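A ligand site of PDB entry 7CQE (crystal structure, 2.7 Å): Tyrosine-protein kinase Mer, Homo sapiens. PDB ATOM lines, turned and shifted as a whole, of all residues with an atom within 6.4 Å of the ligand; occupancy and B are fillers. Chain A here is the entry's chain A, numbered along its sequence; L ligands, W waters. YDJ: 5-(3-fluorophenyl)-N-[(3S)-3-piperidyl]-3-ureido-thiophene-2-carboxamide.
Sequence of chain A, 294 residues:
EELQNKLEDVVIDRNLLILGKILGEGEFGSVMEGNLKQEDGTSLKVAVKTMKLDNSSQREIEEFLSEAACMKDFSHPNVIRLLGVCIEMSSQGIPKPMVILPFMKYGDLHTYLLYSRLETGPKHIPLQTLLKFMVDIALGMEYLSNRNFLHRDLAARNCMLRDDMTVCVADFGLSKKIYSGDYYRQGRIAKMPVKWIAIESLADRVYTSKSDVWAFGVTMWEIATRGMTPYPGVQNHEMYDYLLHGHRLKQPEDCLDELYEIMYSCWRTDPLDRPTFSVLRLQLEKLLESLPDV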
ATOM      1  N   LEU A  23     -28.195 -22.385   0.131  1.00  0.00           N
ATOM      2  CA  LEU A  23     -27.331 -23.328   0.919  1.00  0.00           C
ATOM      3  C   LEU A  23     -27.528 -23.141   2.427  1.00  0.00           C
ATOM      4  O   LEU A  23     -27.099 -24.038   3.187  1.00  0.00           O
ATOM      5  CB  LEU A  23     -25.869 -23.016   0.598  1.00  0.00           C
ATOM      6  CG  LEU A  23     -25.418 -23.294  -0.831  1.00  0.00           C
ATOM      7  CD1 LEU A  23     -24.005 -22.789  -1.042  1.00  0.00           C
ATOM      8  CD2 LEU A  23     -25.543 -24.780  -1.157  1.00  0.00           C
ATOM      9  N   GLY A  24     -28.038 -21.983   2.864  1.00  0.00           N
ATOM     10  CA  GLY A  24     -27.915 -21.496   4.257  1.00  0.00           C
ATOM     11  C   GLY A  24     -28.632 -20.170   4.439  1.00  0.00           C
ATOM     12  O   GLY A  24     -29.264 -19.705   3.458  1.00  0.00           O
ATOM     13  N   GLU A  25     -28.550 -19.609   5.654  1.00  0.00           N
ATOM     14  CA  GLU A  25     -29.263 -18.353   6.062  1.00  0.00           C
ATOM     15  C   GLU A  25     -28.305 -17.465   6.872  1.00  0.00           C
ATOM     16  O   GLU A  25     -28.134 -17.758   8.065  1.00  0.00           O
ATOM     17  CB  GLU A  25     -30.508 -18.659   6.915  1.00  0.00           C
ATOM     18  CG  GLU A  25     -31.501 -19.633   6.296  1.00  0.00           C
ATOM     19  CD  GLU A  25     -32.316 -19.070   5.148  1.00  0.00           C
ATOM     20  OE1 GLU A  25     -31.933 -17.996   4.640  1.00  0.00           O
ATOM     21  OE2 GLU A  25     -33.326 -19.708   4.775  1.00  0.00           O
ATOM     22  N   GLY A  26     -27.721 -16.429   6.244  1.00  0.00           N
ATOM     23  CA  GLY A  26     -26.761 -15.484   6.881  1.00  0.00           C
ATOM     24  C   GLY A  26     -26.452 -14.264   6.027  1.00  0.00           C
ATOM     25  O   GLY A  26     -26.392 -14.436   4.783  1.00  0.00           O
ATOM     26  N   VAL A  31     -27.601 -17.475   1.683  1.00  0.00           N
ATOM     27  CA  VAL A  31     -26.322 -17.823   0.983  1.00  0.00           C
ATOM     28  C   VAL A  31     -26.620 -18.892  -0.083  1.00  0.00           C
ATOM     29  O   VAL A  31     -27.314 -19.875   0.204  1.00  0.00           O
ATOM     30  CB  VAL A  31     -25.200 -18.247   1.950  1.00  0.00           C
ATOM     31  CG1 VAL A  31     -25.680 -19.211   3.020  1.00  0.00           C
ATOM     32  CG2 VAL A  31     -23.985 -18.830   1.226  1.00  0.00           C
ATOM     33  N   VAL A  46     -18.984 -21.014  -6.660  1.00  0.00           N
ATOM     34  CA  VAL A  46     -18.923 -19.935  -5.631  1.00  0.00           C
ATOM     35  C   VAL A  46     -20.136 -20.073  -4.680  1.00  0.00           C
ATOM     36  O   VAL A  46     -21.140 -20.696  -5.037  1.00  0.00           O
ATOM     37  CB  VAL A  46     -18.843 -18.550  -6.301  1.00  0.00           C
ATOM     38  CG1 VAL A  46     -17.513 -18.397  -7.038  1.00  0.00           C
ATOM     39  CG2 VAL A  46     -20.021 -18.264  -7.240  1.00  0.00           C
ATOM     40  N   ALA A  47     -19.992 -19.561  -3.462  1.00  0.00           N
ATOM     41  CA  ALA A  47     -21.171 -19.259  -2.620  1.00  0.00           C
ATOM     42  C   ALA A  47     -21.426 -17.745  -2.753  1.00  0.00           C
ATOM     43  O   ALA A  47     -20.454 -16.966  -2.790  1.00  0.00           O
ATOM     44  CB  ALA A  47     -20.983 -19.711  -1.206  1.00  0.00           C
ATOM     45  N   LYS A  49     -23.524 -14.653  -1.017  1.00  0.00           N
ATOM     46  CA  LYS A  49     -24.313 -14.280   0.178  1.00  0.00           C
ATOM     47  C   LYS A  49     -24.803 -12.841   0.036  1.00  0.00           C
ATOM     48  O   LYS A  49     -23.967 -11.959  -0.153  1.00  0.00           O
ATOM     49  CB  LYS A  49     -23.539 -14.702   1.433  1.00  0.00           C
ATOM     50  CG  LYS A  49     -22.462 -13.770   1.945  1.00  0.00           C
ATOM     51  CD  LYS A  49     -21.949 -14.216   3.292  1.00  0.00           C
ATOM     52  CE  LYS A  49     -23.005 -14.159   4.371  1.00  0.00           C
ATOM     53  NZ  LYS A  49     -23.371 -12.770   4.726  1.00  0.00           N
ATOM     54  N   ILE A  80     -11.213 -16.938   4.745  1.00  0.00           N
ATOM     55  CA  ILE A  80     -11.934 -17.210   3.473  1.00  0.00           C
ATOM     56  C   ILE A  80     -11.598 -16.037   2.559  1.00  0.00           C
ATOM     57  O   ILE A  80     -11.495 -14.927   3.087  1.00  0.00           O
ATOM     58  CB  ILE A  80     -13.451 -17.380   3.698  1.00  0.00           C
ATOM     59  CG1 ILE A  80     -14.096 -18.096   2.516  1.00  0.00           C
ATOM     60  CG2 ILE A  80     -14.148 -16.062   4.018  1.00  0.00           C
ATOM     61  CD1 ILE A  80     -15.474 -18.621   2.838  1.00  0.00           C
ATOM     62  N   LEU A 101     -17.758 -15.799  -2.780  1.00  0.00           N
ATOM     63  CA  LEU A 101     -16.860 -16.620  -1.921  1.00  0.00           C
ATOM     64  C   LEU A 101     -16.625 -17.949  -2.596  1.00  0.00           C
ATOM     65  O   LEU A 101     -17.539 -18.490  -3.219  1.00  0.00           O
ATOM     66  CB  LEU A 101     -17.560 -16.811  -0.574  1.00  0.00           C
ATOM     67  CG  LEU A 101     -17.813 -15.526   0.213  1.00  0.00           C
ATOM     68  CD1 LEU A 101     -19.052 -15.629   1.084  1.00  0.00           C
ATOM     69  CD2 LEU A 101     -16.608 -15.173   1.064  1.00  0.00           C
ATOM     70  N   PRO A 102     -15.453 -18.587  -2.425  1.00  0.00           N
ATOM     71  CA  PRO A 102     -15.238 -19.929  -2.944  1.00  0.00           C
ATOM     72  C   PRO A 102     -16.257 -20.856  -2.277  1.00  0.00           C
ATOM     73  O   PRO A 102     -16.488 -20.703  -1.096  1.00  0.00           O
ATOM     74  CB  PRO A 102     -13.797 -20.289  -2.586  1.00  0.00           C
ATOM     75  CG  PRO A 102     -13.365 -19.276  -1.586  1.00  0.00           C
ATOM     76  CD  PRO A 102     -14.314 -18.091  -1.680  1.00  0.00           C
ATOM     77  N   PHE A 103     -16.883 -21.732  -3.062  1.00  0.00           N
ATOM     78  CA  PHE A 103     -17.857 -22.742  -2.585  1.00  0.00           C
ATOM     79  C   PHE A 103     -17.127 -23.822  -1.774  1.00  0.00           C
ATOM     80  O   PHE A 103     -16.063 -24.276  -2.197  1.00  0.00           O
ATOM     81  CB  PHE A 103     -18.656 -23.345  -3.752  1.00  0.00           C
ATOM     82  CG  PHE A 103     -19.611 -24.434  -3.305  1.00  0.00           C
ATOM     83  CD1 PHE A 103     -20.786 -24.103  -2.641  1.00  0.00           C
ATOM     84  CD2 PHE A 103     -19.288 -25.769  -3.474  1.00  0.00           C
ATOM     85  CE1 PHE A 103     -21.631 -25.093  -2.199  1.00  0.00           C
ATOM     86  CE2 PHE A 103     -20.137 -26.756  -3.008  1.00  0.00           C
ATOM     87  CZ  PHE A 103     -21.311 -26.421  -2.373  1.00  0.00           C
ATOM     88  N   MET A 104     -17.689 -24.203  -0.623  1.00  0.00           N
ATOM     89  CA  MET A 104     -17.122 -25.242   0.273  1.00  0.00           C
ATOM     90  C   MET A 104     -18.171 -26.300   0.588  1.00  0.00           C
ATOM     91  O   MET A 104     -19.005 -26.128   1.437  1.00  0.00           O
ATOM     92  CB  MET A 104     -16.476 -24.603   1.494  1.00  0.00           C
ATOM     93  CG  MET A 104     -15.072 -24.185   1.084  1.00  0.00           C
ATOM     94  SD  MET A 104     -14.259 -23.063   2.171  1.00  0.00           S
ATOM     95  CE  MET A 104     -15.549 -21.831   2.315  1.00  0.00           C
ATOM     96  N   LYS A 105     -18.053 -27.406  -0.125  1.00  0.00           N
ATOM     97  CA  LYS A 105     -18.989 -28.542  -0.106  1.00  0.00           C
ATOM     98  C   LYS A 105     -19.084 -29.115   1.320  1.00  0.00           C
ATOM     99  O   LYS A 105     -20.120 -29.671   1.604  1.00  0.00           O
ATOM    100  CB  LYS A 105     -18.568 -29.586  -1.155  1.00  0.00           C
ATOM    101  CG  LYS A 105     -17.136 -30.093  -1.022  1.00  0.00           C
ATOM    102  CD  LYS A 105     -16.861 -31.241  -1.942  1.00  0.00           C
ATOM    103  CE  LYS A 105     -15.579 -31.944  -1.569  1.00  0.00           C
ATOM    104  NZ  LYS A 105     -15.041 -32.689  -2.734  1.00  0.00           N
ATOM    105  N   TYR A 106     -18.064 -28.953   2.189  1.00  0.00           N
ATOM    106  CA  TYR A 106     -18.041 -29.526   3.560  1.00  0.00           C
ATOM    107  C   TYR A 106     -18.779 -28.643   4.570  1.00  0.00           C
ATOM    108  O   TYR A 106     -18.940 -29.140   5.694  1.00  0.00           O
ATOM    109  CB  TYR A 106     -16.626 -29.776   4.047  1.00  0.00           C
ATOM    110  CG  TYR A 106     -15.992 -30.939   3.331  1.00  0.00           C
ATOM    111  CD1 TYR A 106     -16.730 -32.065   3.011  1.00  0.00           C
ATOM    112  CD2 TYR A 106     -14.663 -30.901   2.957  1.00  0.00           C
ATOM    113  CE1 TYR A 106     -16.157 -33.132   2.336  1.00  0.00           C
ATOM    114  CE2 TYR A 106     -14.078 -31.969   2.310  1.00  0.00           C
ATOM    115  CZ  TYR A 106     -14.816 -33.086   2.001  1.00  0.00           C
ATOM    116  OH  TYR A 106     -14.221 -34.108   1.320  1.00  0.00           O
ATOM    117  N   GLY A 107     -19.230 -27.459   4.152  1.00  0.00           N
ATOM    118  CA  GLY A 107     -20.093 -26.554   4.930  1.00  0.00           C
ATOM    119  C   GLY A 107     -19.445 -26.014   6.196  1.00  0.00           C
ATOM    120  O   GLY A 107     -18.195 -26.077   6.321  1.00  0.00           O
ATOM    121  N   ASP A 108     -20.261 -25.541   7.133  1.00  0.00           N
ATOM    122  CA  ASP A 108     -19.779 -24.929   8.400  1.00  0.00           C
ATOM    123  C   ASP A 108     -19.324 -26.042   9.337  1.00  0.00           C
ATOM    124  O   ASP A 108     -19.875 -27.148   9.282  1.00  0.00           O
ATOM    125  CB  ASP A 108     -20.832 -24.045   9.054  1.00  0.00           C
ATOM    126  CG  ASP A 108     -21.932 -24.890   9.632  1.00  0.00           C
ATOM    127  OD1 ASP A 108     -22.711 -25.451   8.846  1.00  0.00           O
ATOM    128  OD2 ASP A 108     -21.946 -25.062  10.850  1.00  0.00           O
ATOM    129  N   ARG A 157     -20.184 -22.005  13.831  1.00  0.00           N
ATOM    130  CA  ARG A 157     -21.176 -21.967  12.732  1.00  0.00           C
ATOM    131  C   ARG A 157     -20.638 -21.078  11.597  1.00  0.00           C
ATOM    132  O   ARG A 157     -21.109 -21.212  10.446  1.00  0.00           O
ATOM    133  CB  ARG A 157     -22.568 -21.511  13.216  1.00  0.00           C
ATOM    134  CG  ARG A 157     -22.717 -20.000  13.406  1.00  0.00           C
ATOM    135  CD  ARG A 157     -23.978 -19.531  14.131  1.00  0.00           C
ATOM    136  NE  ARG A 157     -23.751 -18.228  14.770  1.00  0.00           N
ATOM    137  CZ  ARG A 157     -23.580 -18.004  16.085  1.00  0.00           C
ATOM    138  NH1 ARG A 157     -23.642 -18.990  16.974  1.00  0.00           N
ATOM    139  NH2 ARG A 157     -23.356 -16.761  16.523  1.00  0.00           N
ATOM    140  N   ASN A 158     -19.695 -20.192  11.917  1.00  0.00           N
ATOM    141  CA  ASN A 158     -19.083 -19.183  11.022  1.00  0.00           C
ATOM    142  C   ASN A 158     -17.660 -19.578  10.652  1.00  0.00           C
ATOM    143  O   ASN A 158     -16.980 -18.747  10.064  1.00  0.00           O
ATOM    144  CB  ASN A 158     -19.030 -17.799  11.681  1.00  0.00           C
ATOM    145  CG  ASN A 158     -20.392 -17.182  11.830  1.00  0.00           C
ATOM    146  OD1 ASN A 158     -21.342 -17.670  11.229  1.00  0.00           O
ATOM    147  ND2 ASN A 158     -20.481 -16.080  12.574  1.00  0.00           N
ATOM    148  N   CYS A 159     -17.213 -20.796  10.991  1.00  0.00           N
ATOM    149  CA  CYS A 159     -15.937 -21.353  10.478  1.00  0.00           C
ATOM    150  C   CYS A 159     -16.253 -22.337   9.340  1.00  0.00           C
ATOM    151  O   CYS A 159     -17.126 -23.196   9.529  1.00  0.00           O
ATOM    152  CB  CYS A 159     -15.127 -21.951  11.617  1.00  0.00           C
ATOM    153  SG  CYS A 159     -14.690 -20.714  12.874  1.00  0.00           S
ATOM    154  N   MET A 160     -15.643 -22.184   8.175  1.00  0.00           N
ATOM    155  CA  MET A 160     -15.932 -23.026   6.979  1.00  0.00           C
ATOM    156  C   MET A 160     -14.842 -24.099   6.850  1.00  0.00           C
ATOM    157  O   MET A 160     -13.700 -23.801   7.223  1.00  0.00           O
ATOM    158  CB  MET A 160     -15.983 -22.184   5.717  1.00  0.00           C
ATOM    159  CG  MET A 160     -17.046 -21.101   5.771  1.00  0.00           C
ATOM    160  SD  MET A 160     -18.685 -21.728   6.137  1.00  0.00           S
ATOM    161  CE  MET A 160     -18.866 -22.954   4.859  1.00  0.00           C
ATOM    162  N   ASP A 171     -17.795 -15.173   7.462  1.00  0.00           N
ATOM    163  CA  ASP A 171     -19.024 -14.425   7.864  1.00  0.00           C
ATOM    164  C   ASP A 171     -18.645 -13.230   8.729  1.00  0.00           C
ATOM    165  O   ASP A 171     -19.368 -12.984   9.696  1.00  0.00           O
ATOM    166  CB  ASP A 171     -20.060 -15.349   8.529  1.00  0.00           C
ATOM    167  CG  ASP A 171     -20.861 -16.219   7.539  1.00  0.00           C
ATOM    168  OD1 ASP A 171     -20.592 -16.188   6.313  1.00  0.00           O
ATOM    169  OD2 ASP A 171     -21.762 -16.914   7.982  1.00  0.00           O
HETATM  170  C1  YDJ L   1     -22.373 -27.537   1.001  1.00  0.00           C
HETATM  171  C2  YDJ L   1     -22.036 -26.254   1.424  1.00  0.00           C
HETATM  172  C3  YDJ L   1     -22.854 -25.458   2.223  1.00  0.00           C
HETATM  173  C4  YDJ L   1     -24.042 -25.996   2.608  1.00  0.00           C
HETATM  174  C5  YDJ L   1     -24.380 -27.263   2.208  1.00  0.00           C
HETATM  175  C6  YDJ L   1     -23.564 -28.050   1.421  1.00  0.00           C
HETATM  176  F1  YDJ L   1     -25.534 -27.669   2.605  1.00  0.00           F
HETATM  177  C7  YDJ L   1     -22.542 -24.208   2.616  1.00  0.00           C
HETATM  178  C8  YDJ L   1     -21.627 -23.405   2.024  1.00  0.00           C
HETATM  179  C9  YDJ L   1     -21.515 -22.173   2.569  1.00  0.00           C
HETATM  180  C10 YDJ L   1     -22.312 -21.982   3.651  1.00  0.00           C
HETATM  181  S1  YDJ L   1     -23.224 -23.403   3.878  1.00  0.00           S
HETATM  182  C11 YDJ L   1     -22.370 -20.841   4.428  1.00  0.00           C
HETATM  183  O1  YDJ L   1     -21.787 -19.794   4.099  1.00  0.00           O
HETATM  184  N1  YDJ L   1     -23.077 -20.982   5.581  1.00  0.00           N
HETATM  185  C12 YDJ L   1     -23.152 -19.929   6.641  1.00  0.00           C
HETATM  186  C13 YDJ L   1     -24.581 -19.609   7.056  1.00  0.00           C
HETATM  187  C14 YDJ L   1     -24.472 -18.437   7.932  1.00  0.00           C
HETATM  188  C15 YDJ L   1     -23.672 -18.825   9.216  1.00  0.00           C
HETATM  189  N2  YDJ L   1     -22.364 -19.454   8.959  1.00  0.00           N
HETATM  190  C16 YDJ L   1     -22.397 -20.464   7.880  1.00  0.00           C
HETATM  191  N3  YDJ L   1     -20.646 -21.258   2.174  1.00  0.00           N
HETATM  192  C17 YDJ L   1     -19.610 -21.507   1.347  1.00  0.00           C
HETATM  193  O2  YDJ L   1     -19.500 -22.487   0.648  1.00  0.00           O
HETATM  194  N4  YDJ L   1     -18.706 -20.557   1.279  1.00  0.00           N
HETATM  195  O   HOH W   1     -19.452 -18.180   3.950  1.00  0.00           O
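O of Arg 157 sits at hydrogen-bond distance from N2 of the ligand, at 2.6 Å.
The side-chain carboxylate (OD2) of Asp 171 lies within salt-bridge range of a nitrogen (N2) of the ligand.
The backbone NH of Met 104 is in hydrogen-bond range of an oxygen (O2) of the ligand (2.8 Å).
OD1 of Asn 158 sits at hydrogen-bond distance from N2 of the ligand, at 3.1 Å.
A nitrogen (N4) of the ligand is in hydrogen-bond range of the backbone carbonyl oxygen (O) of Pro 102 (3.3 Å).
Water W1 bridges O1 of the ligand and OD1 of Asp 171.
Leu 23 touches the ligand (O to C4, 3.7 Å).
O of Glu 25 touches C14 of the ligand (3.7 Å).
Gly 26 touches the ligand (CA to C14, 3.9 Å).
Val 31 touches the ligand.
Ala 47 touches the ligand.
CA of Phe 103 touches O2 of the ligand (3.6 Å).
Lys 105 touches the ligand.
Met 160 touches the ligand (CE to C9, 3.6 Å).
Within 4 Å of the ligand: Leu 23, Glu 25, Gly 26, Val 31, Ala 47, Pro 102, Phe 103, Met 104, Lys 105, Arg 157, Asn 158, Met 160 and Asp 171.
The nearest printed residue that does not touch the ligand is Gly 107 (4.02 Å).
OD2 of Asp 171 sits close to OD1 of Asn 158, at 3.4 Å.
O of Leu 101 sits at hydrogen-bond distance from N of Ala 47 (2.7 Å).
N of Leu 23 sits at hydrogen-bond distance from O of Val 31, 2.7 Å away.
O of Gly 24 is in hydrogen-bond range of N of Val 31, 3.3 Å away.
The backbone carbonyl oxygen of Gly 26 sits close to the side-chain amino group of Lys 49 (3.5 Å).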
